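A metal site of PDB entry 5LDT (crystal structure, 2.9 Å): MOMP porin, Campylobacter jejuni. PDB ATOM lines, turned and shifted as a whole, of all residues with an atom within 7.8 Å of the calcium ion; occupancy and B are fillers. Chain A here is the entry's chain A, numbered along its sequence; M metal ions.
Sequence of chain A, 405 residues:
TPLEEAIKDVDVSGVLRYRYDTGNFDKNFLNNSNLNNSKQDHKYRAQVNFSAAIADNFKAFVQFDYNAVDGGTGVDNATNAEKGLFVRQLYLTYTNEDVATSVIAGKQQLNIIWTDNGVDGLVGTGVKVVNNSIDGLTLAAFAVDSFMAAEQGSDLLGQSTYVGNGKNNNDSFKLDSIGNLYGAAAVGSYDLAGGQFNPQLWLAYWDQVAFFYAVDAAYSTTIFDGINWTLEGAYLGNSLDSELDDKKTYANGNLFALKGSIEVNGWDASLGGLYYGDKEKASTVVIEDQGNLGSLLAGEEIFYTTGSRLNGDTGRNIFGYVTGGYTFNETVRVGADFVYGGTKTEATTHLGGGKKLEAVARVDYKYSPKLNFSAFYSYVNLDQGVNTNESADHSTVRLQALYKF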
ATOM      1  N   ARG A  45     -27.906   8.254  13.377  1.00  0.00           N
ATOM      2  CA  ARG A  45     -27.439   6.880  13.308  1.00  0.00           C
ATOM      3  C   ARG A  45     -26.102   6.801  13.982  1.00  0.00           C
ATOM      4  O   ARG A  45     -25.163   7.422  13.517  1.00  0.00           O
ATOM      5  CB  ARG A  45     -27.362   6.358  11.853  1.00  0.00           C
ATOM      6  CG  ARG A  45     -27.109   4.844  11.702  1.00  0.00           C
ATOM      7  CD  ARG A  45     -28.258   4.022  12.264  1.00  0.00           C
ATOM      8  NE  ARG A  45     -28.074   2.580  12.082  1.00  0.00           N
ATOM      9  CZ  ARG A  45     -28.424   1.851  11.018  1.00  0.00           C
ATOM     10  NH1 ARG A  45     -28.963   2.406   9.954  1.00  0.00           N
ATOM     11  NH2 ARG A  45     -28.239   0.522  11.022  1.00  0.00           N
ATOM     12  N   ARG A  88     -26.413  -5.015  17.746  1.00  0.00           N
ATOM     13  CA  ARG A  88     -26.591  -5.227  16.314  1.00  0.00           C
ATOM     14  C   ARG A  88     -25.704  -6.357  15.743  1.00  0.00           C
ATOM     15  O   ARG A  88     -26.076  -7.046  14.808  1.00  0.00           O
ATOM     16  CB  ARG A  88     -26.206  -3.942  15.571  1.00  0.00           C
ATOM     17  CG  ARG A  88     -26.540  -3.950  14.109  1.00  0.00           C
ATOM     18  CD  ARG A  88     -26.566  -2.558  13.519  1.00  0.00           C
ATOM     19  NE  ARG A  88     -27.121  -2.588  12.187  1.00  0.00           N
ATOM     20  CZ  ARG A  88     -26.456  -2.821  11.042  1.00  0.00           C
ATOM     21  NH1 ARG A  88     -25.157  -3.079  11.020  1.00  0.00           N
ATOM     22  NH2 ARG A  88     -27.135  -2.774   9.878  1.00  0.00           N
ATOM     23  N   THR A 115     -24.997  -7.064  -0.738  1.00  0.00           N
ATOM     24  CA  THR A 115     -25.516  -6.286   0.385  1.00  0.00           C
ATOM     25  C   THR A 115     -24.692  -5.006   0.617  1.00  0.00           C
ATOM     26  O   THR A 115     -23.532  -4.898   0.274  1.00  0.00           O
ATOM     27  CB  THR A 115     -25.527  -7.090   1.704  1.00  0.00           C
ATOM     28  OG1 THR A 115     -24.200  -7.457   2.071  1.00  0.00           O
ATOM     29  CG2 THR A 115     -26.374  -8.327   1.565  1.00  0.00           C
ATOM     30  N   ASP A 116     -25.337  -4.045   1.231  1.00  0.00           N
ATOM     31  CA  ASP A 116     -24.664  -2.824   1.664  1.00  0.00           C
ATOM     32  C   ASP A 116     -23.546  -3.256   2.646  1.00  0.00           C
ATOM     33  O   ASP A 116     -23.742  -4.069   3.568  1.00  0.00           O
ATOM     34  CB  ASP A 116     -25.710  -1.841   2.229  1.00  0.00           C
ATOM     35  CG  ASP A 116     -25.142  -0.530   2.677  1.00  0.00           C
ATOM     36  OD1 ASP A 116     -23.959  -0.261   2.446  1.00  0.00           O
ATOM     37  OD2 ASP A 116     -25.928   0.243   3.282  1.00  0.00           O
ATOM     38  N   GLY A 118     -21.751  -0.781   4.200  1.00  0.00           N
ATOM     39  CA  GLY A 118     -21.553   0.404   5.045  1.00  0.00           C
ATOM     40  C   GLY A 118     -22.361   0.384   6.309  1.00  0.00           C
ATOM     41  O   GLY A 118     -22.650  -0.701   6.874  1.00  0.00           O
ATOM     42  N   VAL A 119     -22.780   1.558   6.761  1.00  0.00           N
ATOM     43  CA  VAL A 119     -23.490   1.670   8.037  1.00  0.00           C
ATOM     44  C   VAL A 119     -24.716   0.711   8.169  1.00  0.00           C
ATOM     45  O   VAL A 119     -24.864   0.002   9.151  1.00  0.00           O
ATOM     46  CB  VAL A 119     -23.881   3.122   8.274  1.00  0.00           C
ATOM     47  CG1 VAL A 119     -24.838   3.259   9.435  1.00  0.00           C
ATOM     48  CG2 VAL A 119     -22.641   3.962   8.481  1.00  0.00           C
ATOM     49  N   ASP A 120     -25.566   0.692   7.135  1.00  0.00           N
ATOM     50  CA  ASP A 120     -26.862  -0.008   7.189  1.00  0.00           C
ATOM     51  C   ASP A 120     -26.838  -1.339   6.364  1.00  0.00           C
ATOM     52  O   ASP A 120     -27.811  -1.668   5.721  1.00  0.00           O
ATOM     53  CB  ASP A 120     -27.965   0.918   6.695  1.00  0.00           C
ATOM     54  CG  ASP A 120     -29.334   0.481   7.102  1.00  0.00           C
ATOM     55  OD1 ASP A 120     -29.500   0.112   8.226  1.00  0.00           O
ATOM     56  OD2 ASP A 120     -30.312   0.534   6.332  1.00  0.00           O
ATOM     57  N   GLY A 121     -25.737  -2.086   6.475  1.00  0.00           N
ATOM     58  CA  GLY A 121     -25.568  -3.361   5.775  1.00  0.00           C
ATOM     59  C   GLY A 121     -26.306  -4.512   6.446  1.00  0.00           C
ATOM     60  O   GLY A 121     -26.475  -4.521   7.677  1.00  0.00           O
ATOM     61  N   LEU A 122     -26.781  -5.460   5.641  1.00  0.00           N
ATOM     62  CA  LEU A 122     -27.570  -6.559   6.156  1.00  0.00           C
ATOM     63  C   LEU A 122     -26.768  -7.395   7.105  1.00  0.00           C
ATOM     64  O   LEU A 122     -25.598  -7.716   6.830  1.00  0.00           O
ATOM     65  CB  LEU A 122     -28.128  -7.444   5.035  1.00  0.00           C
ATOM     66  CG  LEU A 122     -28.940  -8.678   5.456  1.00  0.00           C
ATOM     67  CD1 LEU A 122     -30.278  -8.266   6.055  1.00  0.00           C
ATOM     68  CD2 LEU A 122     -29.186  -9.598   4.263  1.00  0.00           C
ATOM     69  N   GLU A 151     -35.103  -5.032  10.727  1.00  0.00           N
ATOM     70  CA  GLU A 151     -34.295  -3.820  10.755  1.00  0.00           C
ATOM     71  C   GLU A 151     -34.145  -3.190   9.360  1.00  0.00           C
ATOM     72  O   GLU A 151     -33.989  -1.968   9.220  1.00  0.00           O
ATOM     73  CB  GLU A 151     -32.867  -4.121  11.247  1.00  0.00           C
ATOM     74  CG  GLU A 151     -32.045  -2.887  11.633  1.00  0.00           C
ATOM     75  CD  GLU A 151     -30.541  -2.979  11.361  1.00  0.00           C
ATOM     76  OE1 GLU A 151     -30.097  -3.542  10.327  1.00  0.00           O
ATOM     77  OE2 GLU A 151     -29.776  -2.371  12.149  1.00  0.00           O
ATOM     78  N   GLN A 152     -34.075  -4.035   8.341  1.00  0.00           N
ATOM     79  CA  GLN A 152     -33.838  -3.595   6.990  1.00  0.00           C
ATOM     80  C   GLN A 152     -35.099  -3.142   6.245  1.00  0.00           C
ATOM     81  O   GLN A 152     -34.995  -2.398   5.245  1.00  0.00           O
ATOM     82  CB  GLN A 152     -33.088  -4.709   6.249  1.00  0.00           C
ATOM     83  CG  GLN A 152     -31.671  -4.883   6.773  1.00  0.00           C
ATOM     84  CD  GLN A 152     -30.855  -3.615   6.580  1.00  0.00           C
ATOM     85  OE1 GLN A 152     -31.008  -2.926   5.555  1.00  0.00           O
ATOM     86  NE2 GLN A 152     -29.968  -3.304   7.512  1.00  0.00           N
ATOM     87  N   GLY A 153     -36.290  -3.513   6.726  1.00  0.00           N
ATOM     88  CA  GLY A 153     -37.516  -3.053   6.154  1.00  0.00           C
ATOM     89  C   GLY A 153     -37.510  -3.328   4.674  1.00  0.00           C
ATOM     90  O   GLY A 153     -37.274  -4.420   4.259  1.00  0.00           O
ATOM     91  N   SER A 154     -37.664  -2.282   3.868  1.00  0.00           N
ATOM     92  CA  SER A 154     -37.812  -2.412   2.427  1.00  0.00           C
ATOM     93  C   SER A 154     -36.462  -2.475   1.702  1.00  0.00           C
ATOM     94  O   SER A 154     -36.439  -2.659   0.483  1.00  0.00           O
ATOM     95  CB  SER A 154     -38.704  -1.311   1.854  1.00  0.00           C
ATOM     96  OG  SER A 154     -38.049  -0.063   1.837  1.00  0.00           O
ATOM     97  N   ASP A 155     -35.349  -2.350   2.437  1.00  0.00           N
ATOM     98  CA  ASP A 155     -34.039  -2.581   1.857  1.00  0.00           C
ATOM     99  C   ASP A 155     -33.890  -4.074   1.455  1.00  0.00           C
ATOM    100  O   ASP A 155     -33.168  -4.401   0.511  1.00  0.00           O
ATOM    101  CB  ASP A 155     -32.896  -2.197   2.804  1.00  0.00           C
ATOM    102  CG  ASP A 155     -32.546  -0.711   2.776  1.00  0.00           C
ATOM    103  OD1 ASP A 155     -33.346   0.151   2.374  1.00  0.00           O
ATOM    104  OD2 ASP A 155     -31.420  -0.402   3.184  1.00  0.00           O
ATOM    105  N   LEU A 156     -34.605  -4.967   2.135  1.00  0.00           N
ATOM    106  CA  LEU A 156     -34.418  -6.364   1.836  1.00  0.00           C
ATOM    107  C   LEU A 156     -35.298  -6.816   0.709  1.00  0.00           C
ATOM    108  O   LEU A 156     -36.494  -6.492   0.656  1.00  0.00           O
ATOM    109  CB  LEU A 156     -34.698  -7.211   3.087  1.00  0.00           C
ATOM    110  CG  LEU A 156     -34.326  -8.699   2.983  1.00  0.00           C
ATOM    111  CD1 LEU A 156     -32.839  -8.913   2.856  1.00  0.00           C
ATOM    112  CD2 LEU A 156     -34.818  -9.418   4.227  1.00  0.00           C
ATOM    113  N   GLU A 288     -29.896  -6.966  -0.587  1.00  0.00           N
ATOM    114  CA  GLU A 288     -30.247  -5.816   0.210  1.00  0.00           C
ATOM    115  C   GLU A 288     -29.780  -4.489  -0.439  1.00  0.00           C
ATOM    116  O   GLU A 288     -28.619  -4.349  -0.809  1.00  0.00           O
ATOM    117  CB  GLU A 288     -29.634  -5.988   1.586  1.00  0.00           C
ATOM    118  CG  GLU A 288     -30.000  -4.877   2.577  1.00  0.00           C
ATOM    119  CD  GLU A 288     -28.883  -3.850   2.834  1.00  0.00           C
ATOM    120  OE1 GLU A 288     -27.721  -4.274   2.883  1.00  0.00           O
ATOM    121  OE2 GLU A 288     -29.200  -2.679   3.109  1.00  0.00           O
ATOM    122  N   ASP A 289     -30.725  -3.548  -0.523  1.00  0.00           N
ATOM    123  CA  ASP A 289     -30.567  -2.182  -0.995  1.00  0.00           C
ATOM    124  C   ASP A 289     -29.984  -2.090  -2.410  1.00  0.00           C
ATOM    125  O   ASP A 289     -30.713  -2.361  -3.367  1.00  0.00           O
ATOM    126  CB  ASP A 289     -29.877  -1.244   0.032  1.00  0.00           C
ATOM    127  CG  ASP A 289     -30.143   0.300  -0.249  1.00  0.00           C
ATOM    128  OD1 ASP A 289     -30.621   0.724  -1.366  1.00  0.00           O
ATOM    129  OD2 ASP A 289     -29.829   1.113   0.659  1.00  0.00           O
ATOM    130  N   GLN A 290     -28.717  -1.676  -2.547  1.00  0.00           N
ATOM    131  CA  GLN A 290     -28.051  -1.683  -3.849  1.00  0.00           C
ATOM    132  C   GLN A 290     -26.753  -2.468  -3.778  1.00  0.00           C
ATOM    133  O   GLN A 290     -25.815  -2.209  -4.528  1.00  0.00           O
ATOM    134  CB  GLN A 290     -27.799  -0.235  -4.260  1.00  0.00           C
ATOM    135  CG  GLN A 290     -29.075   0.589  -4.248  1.00  0.00           C
ATOM    136  CD  GLN A 290     -28.886   2.024  -4.690  1.00  0.00           C
ATOM    137  OE1 GLN A 290     -27.952   2.702  -4.255  1.00  0.00           O
ATOM    138  NE2 GLN A 290     -29.840   2.509  -5.497  1.00  0.00           N
HETATM  139 CA    CA M   1     -29.847  -1.131   4.708  1.00  0.00          CA
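N of Asp 289 sits at hydrogen-bond distance from O of Asp 155 (2.8 Å). The side-chain carboxylate (OE1) of Glu 288 lies within hydrogen-bond range of the backbone NH (N) of Leu 122, at 3.1 Å. The side-chain carboxylate (OD1) of Asp 120 lies within salt-bridge range of the guanidinium group (NH1) of Arg 45 (2.9 Å). The side-chain amide nitrogen (NE2) of Gln 152 lies within hydrogen-bond range of the side-chain carboxylate (OE1) of Glu 151 (2.8 Å). OE1 of Glu 288 is in hydrogen-bond range of N of Asp 116 (2.9 Å).
The calcium ion is bound by the side-chain amide oxygen of Gln 152 (2.3 Å), the side-chain carboxylate of Asp 155 (2.3 Å), the side-chain carboxylate of Glu 288 (2.3 Å), the backbone carbonyl oxygen of Asp 120 (2.3 Å) and the side-chain carboxylate of Asp 120 (2.4 Å).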
